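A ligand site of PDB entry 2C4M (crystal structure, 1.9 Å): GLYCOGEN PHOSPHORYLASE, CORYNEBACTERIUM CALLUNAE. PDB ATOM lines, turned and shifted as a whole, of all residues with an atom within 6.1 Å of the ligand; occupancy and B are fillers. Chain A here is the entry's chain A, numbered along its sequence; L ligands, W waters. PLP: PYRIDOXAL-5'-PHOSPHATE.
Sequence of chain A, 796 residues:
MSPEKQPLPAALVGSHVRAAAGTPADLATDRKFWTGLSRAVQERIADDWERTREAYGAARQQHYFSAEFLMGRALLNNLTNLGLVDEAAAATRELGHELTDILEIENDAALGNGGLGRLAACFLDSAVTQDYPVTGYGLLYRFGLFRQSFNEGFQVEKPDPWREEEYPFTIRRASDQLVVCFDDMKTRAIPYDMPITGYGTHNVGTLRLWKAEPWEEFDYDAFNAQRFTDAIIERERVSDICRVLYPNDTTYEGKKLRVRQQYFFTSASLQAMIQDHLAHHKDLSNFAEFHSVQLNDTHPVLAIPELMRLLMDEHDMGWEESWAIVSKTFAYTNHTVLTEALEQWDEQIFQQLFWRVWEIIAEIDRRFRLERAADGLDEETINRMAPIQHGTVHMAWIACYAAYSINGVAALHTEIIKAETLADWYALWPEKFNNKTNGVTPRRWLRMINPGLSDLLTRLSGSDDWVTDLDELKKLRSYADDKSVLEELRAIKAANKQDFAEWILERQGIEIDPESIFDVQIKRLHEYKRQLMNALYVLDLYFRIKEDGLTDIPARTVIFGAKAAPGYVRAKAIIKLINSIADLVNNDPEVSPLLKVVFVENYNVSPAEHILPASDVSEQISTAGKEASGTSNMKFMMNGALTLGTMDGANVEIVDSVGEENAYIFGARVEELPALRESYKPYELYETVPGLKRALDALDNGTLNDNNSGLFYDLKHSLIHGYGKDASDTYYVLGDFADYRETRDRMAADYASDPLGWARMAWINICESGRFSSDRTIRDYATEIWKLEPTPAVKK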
ATOM      1  N   LEU A  70      19.451   4.409 -19.009  1.00  0.00           N
ATOM      2  CA  LEU A  70      19.741   5.637 -19.737  1.00  0.00           C
ATOM      3  C   LEU A  70      19.326   5.408 -21.183  1.00  0.00           C
ATOM      4  O   LEU A  70      20.156   5.222 -22.073  1.00  0.00           O
ATOM      5  CB  LEU A  70      21.234   5.958 -19.644  1.00  0.00           C
ATOM      6  CG  LEU A  70      21.594   7.401 -19.988  1.00  0.00           C
ATOM      7  CD1 LEU A  70      20.979   8.354 -18.952  1.00  0.00           C
ATOM      8  CD2 LEU A  70      23.094   7.537 -20.003  1.00  0.00           C
ATOM      9  N   ASN A 113      21.283   7.635 -15.189  1.00  0.00           N
ATOM     10  CA  ASN A 113      22.245   8.643 -14.819  1.00  0.00           C
ATOM     11  C   ASN A 113      23.538   8.523 -15.640  1.00  0.00           C
ATOM     12  O   ASN A 113      23.899   9.412 -16.400  1.00  0.00           O
ATOM     13  CB  ASN A 113      22.567   8.477 -13.325  1.00  0.00           C
ATOM     14  CG  ASN A 113      23.696   9.405 -12.951  1.00  0.00           C
ATOM     15  OD1 ASN A 113      24.028  10.349 -13.671  1.00  0.00           O
ATOM     16  ND2 ASN A 113      24.290   9.133 -11.783  1.00  0.00           N
ATOM     17  N   GLY A 114      24.262   7.384 -15.476  1.00  0.00           N
ATOM     18  CA  GLY A 114      25.522   7.231 -16.234  1.00  0.00           C
ATOM     19  C   GLY A 114      25.699   5.825 -16.829  1.00  0.00           C
ATOM     20  O   GLY A 114      24.751   5.195 -17.299  1.00  0.00           O
ATOM     21  N   GLY A 115      26.945   5.380 -16.778  1.00  0.00           N
ATOM     22  CA  GLY A 115      27.324   4.077 -17.304  1.00  0.00           C
ATOM     23  C   GLY A 115      26.467   2.900 -16.872  1.00  0.00           C
ATOM     24  O   GLY A 115      26.086   2.088 -17.706  1.00  0.00           O
ATOM     25  N   LEU A 116      26.168   2.807 -15.583  1.00  0.00           N
ATOM     26  CA  LEU A 116      25.356   1.709 -15.102  1.00  0.00           C
ATOM     27  C   LEU A 116      24.042   1.684 -15.858  1.00  0.00           C
ATOM     28  O   LEU A 116      23.580   0.613 -16.283  1.00  0.00           O
ATOM     29  CB  LEU A 116      25.075   1.862 -13.604  1.00  0.00           C
ATOM     30  CG  LEU A 116      24.361   0.679 -12.939  1.00  0.00           C
ATOM     31  CD1 LEU A 116      25.227  -0.571 -13.060  1.00  0.00           C
ATOM     32  CD2 LEU A 116      24.086   0.997 -11.470  1.00  0.00           C
ATOM     33  N   ARG A 118      23.347   3.283 -18.826  1.00  0.00           N
ATOM     34  CA  ARG A 118      23.509   3.111 -20.270  1.00  0.00           C
ATOM     35  C   ARG A 118      23.832   1.663 -20.599  1.00  0.00           C
ATOM     36  O   ARG A 118      23.549   1.200 -21.704  1.00  0.00           O
ATOM     37  CB  ARG A 118      24.599   4.038 -20.814  1.00  0.00           C
ATOM     38  CG  ARG A 118      24.764   3.940 -22.329  1.00  0.00           C
ATOM     39  CD  ARG A 118      23.440   4.177 -23.059  1.00  0.00           C
ATOM     40  NE  ARG A 118      23.169   3.119 -24.033  1.00  0.00           N
ATOM     41  CZ  ARG A 118      22.100   3.077 -24.815  1.00  0.00           C
ATOM     42  NH1 ARG A 118      21.185   4.035 -24.760  1.00  0.00           N
ATOM     43  NH2 ARG A 118      21.943   2.069 -25.669  1.00  0.00           N
ATOM     44  N   VAL A 440      28.830  -2.128 -25.708  1.00  0.00           N
ATOM     45  CA  VAL A 440      27.811  -1.165 -26.090  1.00  0.00           C
ATOM     46  C   VAL A 440      27.110  -1.666 -27.328  1.00  0.00           C
ATOM     47  O   VAL A 440      27.560  -2.619 -27.946  1.00  0.00           O
ATOM     48  CB  VAL A 440      28.512   0.185 -26.367  1.00  0.00           C
ATOM     49  CG1 VAL A 440      29.266   0.668 -25.123  1.00  0.00           C
ATOM     50  CG2 VAL A 440      29.498   0.046 -27.526  1.00  0.00           C
ATOM     51  N   TRP A 445      25.033   3.347 -31.258  1.00  0.00           N
ATOM     52  CA  TRP A 445      26.350   4.010 -31.231  1.00  0.00           C
ATOM     53  C   TRP A 445      27.198   3.929 -32.524  1.00  0.00           C
ATOM     54  O   TRP A 445      28.318   4.429 -32.588  1.00  0.00           O
ATOM     55  CB  TRP A 445      27.156   3.455 -30.049  1.00  0.00           C
ATOM     56  CG  TRP A 445      26.427   3.676 -28.781  1.00  0.00           C
ATOM     57  CD1 TRP A 445      25.882   2.684 -27.953  1.00  0.00           C
ATOM     58  CD2 TRP A 445      26.056   4.952 -28.203  1.00  0.00           C
ATOM     59  NE1 TRP A 445      25.200   3.199 -26.903  1.00  0.00           N
ATOM     60  CE2 TRP A 445      25.294   4.673 -27.046  1.00  0.00           C
ATOM     61  CE3 TRP A 445      26.283   6.283 -28.563  1.00  0.00           C
ATOM     62  CZ2 TRP A 445      24.788   5.707 -26.282  1.00  0.00           C
ATOM     63  CZ3 TRP A 445      25.786   7.320 -27.802  1.00  0.00           C
ATOM     64  CH2 TRP A 445      25.026   7.028 -26.653  1.00  0.00           C
ATOM     65  N   ILE A 522      34.245  13.187 -22.659  1.00  0.00           N
ATOM     66  CA  ILE A 522      32.890  13.137 -22.153  1.00  0.00           C
ATOM     67  C   ILE A 522      32.773  12.097 -21.065  1.00  0.00           C
ATOM     68  O   ILE A 522      32.883  10.898 -21.319  1.00  0.00           O
ATOM     69  CB  ILE A 522      31.949  12.780 -23.315  1.00  0.00           C
ATOM     70  CG1 ILE A 522      32.519  11.615 -24.131  1.00  0.00           C
ATOM     71  CG2 ILE A 522      31.802  13.993 -24.267  1.00  0.00           C
ATOM     72  CD1 ILE A 522      31.582  11.191 -25.258  1.00  0.00           C
ATOM     73  N   LYS A 523      32.722  12.606 -19.837  1.00  0.00           N
ATOM     74  CA  LYS A 523      32.690  11.754 -18.662  1.00  0.00           C
ATOM     75  C   LYS A 523      32.046  12.528 -17.521  1.00  0.00           C
ATOM     76  O   LYS A 523      32.235  13.726 -17.376  1.00  0.00           O
ATOM     77  CB  LYS A 523      34.128  11.382 -18.256  1.00  0.00           C
ATOM     78  CG  LYS A 523      34.926  10.638 -19.345  1.00  0.00           C
ATOM     79  CD  LYS A 523      35.626   9.383 -18.806  1.00  0.00           C
ATOM     80  CE  LYS A 523      35.008   8.089 -19.364  1.00  0.00           C
ATOM     81  NZ  LYS A 523      35.839   6.953 -18.995  1.00  0.00           N
ATOM     82  N   ARG A 524      31.439  11.775 -16.582  1.00  0.00           N
ATOM     83  CA  ARG A 524      31.024  12.421 -15.346  1.00  0.00           C
ATOM     84  C   ARG A 524      32.197  13.191 -14.705  1.00  0.00           C
ATOM     85  O   ARG A 524      33.320  12.716 -14.681  1.00  0.00           O
ATOM     86  CB  ARG A 524      30.540  11.333 -14.387  1.00  0.00           C
ATOM     87  CG  ARG A 524      30.195  11.902 -13.006  1.00  0.00           C
ATOM     88  CD  ARG A 524      29.147  13.010 -13.098  1.00  0.00           C
ATOM     89  NE  ARG A 524      28.122  12.683 -14.088  1.00  0.00           N
ATOM     90  CZ  ARG A 524      27.041  12.015 -13.654  1.00  0.00           C
ATOM     91  NH1 ARG A 524      26.922  11.710 -12.369  1.00  0.00           N
ATOM     92  NH2 ARG A 524      26.101  11.635 -14.524  1.00  0.00           N
ATOM     93  N   LYS A 529      38.707  11.250 -12.480  1.00  0.00           N
ATOM     94  CA  LYS A 529      38.598  11.313 -13.929  1.00  0.00           C
ATOM     95  C   LYS A 529      39.621  12.292 -14.543  1.00  0.00           C
ATOM     96  O   LYS A 529      39.909  12.270 -15.732  1.00  0.00           O
ATOM     97  CB  LYS A 529      37.177  11.739 -14.294  1.00  0.00           C
ATOM     98  CG  LYS A 529      36.388  10.627 -14.980  1.00  0.00           C
ATOM     99  CD  LYS A 529      36.021   9.490 -14.028  1.00  0.00           C
ATOM    100  CE  LYS A 529      34.593   8.960 -14.254  1.00  0.00           C
ATOM    101  NZ  LYS A 529      34.652   7.646 -14.891  1.00  0.00           N
ATOM    102  N   TYR A 603      25.295  17.345 -20.947  1.00  0.00           N
ATOM    103  CA  TYR A 603      25.734  16.136 -21.609  1.00  0.00           C
ATOM    104  C   TYR A 603      24.778  14.976 -21.280  1.00  0.00           C
ATOM    105  O   TYR A 603      24.354  14.793 -20.148  1.00  0.00           O
ATOM    106  CB  TYR A 603      27.152  15.800 -21.157  1.00  0.00           C
ATOM    107  CG  TYR A 603      27.641  14.484 -21.670  1.00  0.00           C
ATOM    108  CD1 TYR A 603      27.875  14.288 -23.033  1.00  0.00           C
ATOM    109  CD2 TYR A 603      27.871  13.427 -20.794  1.00  0.00           C
ATOM    110  CE1 TYR A 603      28.323  13.052 -23.513  1.00  0.00           C
ATOM    111  CE2 TYR A 603      28.323  12.198 -21.255  1.00  0.00           C
ATOM    112  CZ  TYR A 603      28.553  12.010 -22.621  1.00  0.00           C
ATOM    113  OH  TYR A 603      28.997  10.799 -23.087  1.00  0.00           O
ATOM    114  N   ASN A 604      24.428  14.217 -22.315  1.00  0.00           N
ATOM    115  CA  ASN A 604      23.511  13.101 -22.143  1.00  0.00           C
ATOM    116  C   ASN A 604      23.623  12.230 -23.391  1.00  0.00           C
ATOM    117  O   ASN A 604      24.520  12.426 -24.198  1.00  0.00           O
ATOM    118  CB  ASN A 604      22.069  13.608 -21.955  1.00  0.00           C
ATOM    119  CG  ASN A 604      21.199  12.635 -21.160  1.00  0.00           C
ATOM    120  OD1 ASN A 604      21.283  11.419 -21.348  1.00  0.00           O
ATOM    121  ND2 ASN A 604      20.354  13.174 -20.289  1.00  0.00           N
ATOM    122  N   VAL A 605      22.705  11.291 -23.535  1.00  0.00           N
ATOM    123  CA  VAL A 605      22.711  10.393 -24.696  1.00  0.00           C
ATOM    124  C   VAL A 605      22.670  11.130 -26.040  1.00  0.00           C
ATOM    125  O   VAL A 605      23.477  10.852 -26.934  1.00  0.00           O
ATOM    126  CB  VAL A 605      21.543   9.393 -24.631  1.00  0.00           C
ATOM    127  CG1 VAL A 605      21.555   8.460 -25.845  1.00  0.00           C
ATOM    128  CG2 VAL A 605      21.654   8.557 -23.353  1.00  0.00           C
ATOM    129  N   SER A 606      21.721  12.062 -26.197  1.00  0.00           N
ATOM    130  CA  SER A 606      21.605  12.790 -27.444  1.00  0.00           C
ATOM    131  C   SER A 606      22.910  13.534 -27.772  1.00  0.00           C
ATOM    132  O   SER A 606      23.409  13.458 -28.901  1.00  0.00           O
ATOM    133  CB  SER A 606      20.430  13.772 -27.395  1.00  0.00           C
ATOM    134  OG  SER A 606      20.067  14.160 -28.712  1.00  0.00           O
ATOM    135  N   ALA A 608      25.890  12.847 -26.796  1.00  0.00           N
ATOM    136  CA  ALA A 608      26.893  11.827 -27.109  1.00  0.00           C
ATOM    137  C   ALA A 608      26.733  11.365 -28.558  1.00  0.00           C
ATOM    138  O   ALA A 608      27.723  11.144 -29.263  1.00  0.00           O
ATOM    139  CB  ALA A 608      26.724  10.633 -26.169  1.00  0.00           C
ATOM    140  N   LEU A 612      30.366  11.774 -30.686  1.00  0.00           N
ATOM    141  CA  LEU A 612      31.141  10.605 -31.067  1.00  0.00           C
ATOM    142  C   LEU A 612      31.557  10.456 -32.532  1.00  0.00           C
ATOM    143  O   LEU A 612      32.728  10.218 -32.814  1.00  0.00           O
ATOM    144  CB  LEU A 612      30.406   9.348 -30.599  1.00  0.00           C
ATOM    145  CG  LEU A 612      30.328   9.194 -29.075  1.00  0.00           C
ATOM    146  CD1 LEU A 612      29.134   8.356 -28.694  1.00  0.00           C
ATOM    147  CD2 LEU A 612      31.600   8.554 -28.565  1.00  0.00           C
ATOM    148  N   GLN A 620      40.628   9.263 -22.186  1.00  0.00           N
ATOM    149  CA  GLN A 620      40.297   8.337 -21.103  1.00  0.00           C
ATOM    150  C   GLN A 620      41.420   8.323 -20.073  1.00  0.00           C
ATOM    151  O   GLN A 620      42.210   7.391 -19.978  1.00  0.00           O
ATOM    152  CB  GLN A 620      40.105   6.950 -21.700  1.00  0.00           C
ATOM    153  CG  GLN A 620      39.125   6.944 -22.885  1.00  0.00           C
ATOM    154  CD  GLN A 620      37.733   7.228 -22.386  1.00  0.00           C
ATOM    155  OE1 GLN A 620      37.403   7.099 -21.219  1.00  0.00           O
ATOM    156  NE2 GLN A 620      36.880   7.637 -23.351  1.00  0.00           N
ATOM    157  N   SER A 629      35.810  -0.363 -15.920  1.00  0.00           N
ATOM    158  CA  SER A 629      35.376  -0.536 -17.295  1.00  0.00           C
ATOM    159  C   SER A 629      35.630   0.714 -18.133  1.00  0.00           C
ATOM    160  O   SER A 629      36.726   1.265 -18.179  1.00  0.00           O
ATOM    161  CB  SER A 629      33.883  -0.890 -17.300  1.00  0.00           C
ATOM    162  OG  SER A 629      33.470  -1.284 -18.598  1.00  0.00           O
ATOM    163  N   GLY A 630      34.575   1.152 -18.846  1.00  0.00           N
ATOM    164  CA  GLY A 630      34.709   2.336 -19.676  1.00  0.00           C
ATOM    165  C   GLY A 630      33.993   2.142 -21.013  1.00  0.00           C
ATOM    166  O   GLY A 630      34.612   2.007 -22.060  1.00  0.00           O
ATOM    167  N   THR A 631      32.639   2.165 -20.960  1.00  0.00           N
ATOM    168  CA  THR A 631      31.893   1.939 -22.192  1.00  0.00           C
ATOM    169  C   THR A 631      31.985   3.104 -23.191  1.00  0.00           C
ATOM    170  O   THR A 631      31.922   2.890 -24.394  1.00  0.00           O
ATOM    171  CB  THR A 631      30.437   1.653 -21.838  1.00  0.00           C
ATOM    172  OG1 THR A 631      29.909   2.726 -21.062  1.00  0.00           O
ATOM    173  CG2 THR A 631      30.345   0.355 -21.040  1.00  0.00           C
ATOM    174  N   SER A 632      32.111   4.357 -22.726  1.00  0.00           N
ATOM    175  CA  SER A 632      32.223   5.452 -23.681  1.00  0.00           C
ATOM    176  C   SER A 632      33.505   5.234 -24.507  1.00  0.00           C
ATOM    177  O   SER A 632      33.568   5.574 -25.693  1.00  0.00           O
ATOM    178  CB  SER A 632      32.289   6.819 -22.983  1.00  0.00           C
ATOM    179  OG  SER A 632      33.449   6.965 -22.184  1.00  0.00           O
ATOM    180  N   ASN A 633      34.517   4.648 -23.849  1.00  0.00           N
ATOM    181  CA  ASN A 633      35.794   4.351 -24.492  1.00  0.00           C
ATOM    182  C   ASN A 633      35.507   3.518 -25.742  1.00  0.00           C
ATOM    183  O   ASN A 633      36.039   3.768 -26.815  1.00  0.00           O
ATOM    184  CB  ASN A 633      36.699   3.523 -23.568  1.00  0.00           C
ATOM    185  CG  ASN A 633      36.861   4.128 -22.184  1.00  0.00           C
ATOM    186  OD1 ASN A 633      35.883   4.532 -21.538  1.00  0.00           O
ATOM    187  ND2 ASN A 633      38.104   4.175 -21.693  1.00  0.00           N
ATOM    188  N   LYS A 635      32.658   3.243 -27.447  1.00  0.00           N
ATOM    189  CA  LYS A 635      31.870   3.943 -28.458  1.00  0.00           C
ATOM    190  C   LYS A 635      32.778   4.785 -29.344  1.00  0.00           C
ATOM    191  O   LYS A 635      32.560   4.896 -30.546  1.00  0.00           O
ATOM    192  CB  LYS A 635      30.832   4.841 -27.776  1.00  0.00           C
ATOM    193  CG  LYS A 635      29.961   4.074 -26.806  1.00  0.00           C
ATOM    194  CD  LYS A 635      28.968   4.981 -26.083  1.00  0.00           C
ATOM    195  CE  LYS A 635      28.255   4.254 -24.945  1.00  0.00           C
ATOM    196  NZ  LYS A 635      27.642   5.230 -24.038  1.00  0.00           N
HETATM  197  N1  PLP L   1      26.655   8.664 -20.245  1.00  0.00           N
HETATM  198  C2  PLP L   1      26.259   8.682 -21.569  1.00  0.00           C
HETATM  199  C2A PLP L   1      25.512   9.820 -22.077  1.00  0.00           C
HETATM  200  C3  PLP L   1      26.717   7.642 -22.440  1.00  0.00           C
HETATM  201  O3  PLP L   1      26.158   7.554 -23.700  1.00  0.00           O
HETATM  202  C4  PLP L   1      27.575   6.677 -21.946  1.00  0.00           C
HETATM  203  C4A PLP L   1      28.040   5.650 -22.910  1.00  0.00           C
HETATM  204  C5  PLP L   1      28.001   6.677 -20.613  1.00  0.00           C
HETATM  205  C6  PLP L   1      27.503   7.691 -19.723  1.00  0.00           C
HETATM  206  C5A PLP L   1      29.069   5.790 -19.987  1.00  0.00           C
HETATM  207  O4P PLP L   1      30.311   6.541 -19.921  1.00  0.00           O
HETATM  208  P   PLP L   1      31.477   6.198 -19.051  1.00  0.00           P
HETATM  209  O1P PLP L   1      31.964   7.595 -18.469  1.00  0.00           O
HETATM  210  O2P PLP L   1      31.159   5.257 -17.791  1.00  0.00           O
HETATM  211  O3P PLP L   1      32.554   5.550 -20.020  1.00  0.00           O
HETATM  212  O   HOH W   1      30.395   9.223 -21.362  1.00  0.00           O
HETATM  213  O   HOH W   2      25.506  10.517 -18.259  1.00  0.00           O
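An oxygen (O3P) of the ligand is in salt-bridge range of the side-chain amino group (NZ) of Lys 523, at 3.7 Å.
The backbone NH (N) of Ser 632 is in hydrogen-bond range of an oxygen (O3P) of the ligand.
An oxygen (O3P) of the ligand lies within hydrogen-bond range of the side-chain hydroxyl (OG) of Ser 632.
NZ of Lys 635 is bonded to C4A of the ligand, 1.3 Å away.
Water W2 lies within hydrogen-bond range of the backbone carbonyl oxygen (O) of Asn 113 (2.7 Å) and a nitrogen (N1) of the ligand (2.9 Å).
Water W1 lies within hydrogen-bond range of OH of Tyr 603 (2.7 Å), O of Ile 522 (3.0 Å) and O4P of the ligand (3.0 Å).
The side-chain amide oxygen (OE1) of Gln 620 is in hydrogen-bond range of the side-chain amino group (NZ) of Lys 523, 2.7 Å away.
The backbone carbonyl oxygen (O) of Gly 630 sits close to the side-chain amide oxygen (OD1) of Asn 633 (2.9 Å).
The side-chain amide oxygen (OE1) of Gln 620 sits close to the side-chain amide oxygen (OD1) of Asn 633.
The backbone carbonyl oxygen (O) of Leu 70 lies within hydrogen-bond range of the guanidinium group (NH1) of Arg 118 (3.1 Å).
Leu 70 touches the ligand (CD2 to C2, 3.7 Å).
Gly 114 touches the ligand (C to C6, 3.9 Å).
CA of Gly 115 touches C5A of the ligand, 3.6 Å away.
CG of Arg 118 touches C4A of the ligand (3.7 Å).
Trp 445 touches the ligand (CH2 to O3, 3.2 Å).
OH of Tyr 603 touches C2A of the ligand, at 3.8 Å.
C of Asn 604 touches C2A of the ligand (3.3 Å).
Val 605 touches the ligand (N to C2A, 3.5 Å).
CB of Ala 608 touches O3 of the ligand, at 3.99 Å.
Gly 630 touches the ligand.
Thr 631 touches the ligand.
Asn 633 touches the ligand.
Of the 25 residues printed, 15 come within 4 Å of the ligand.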
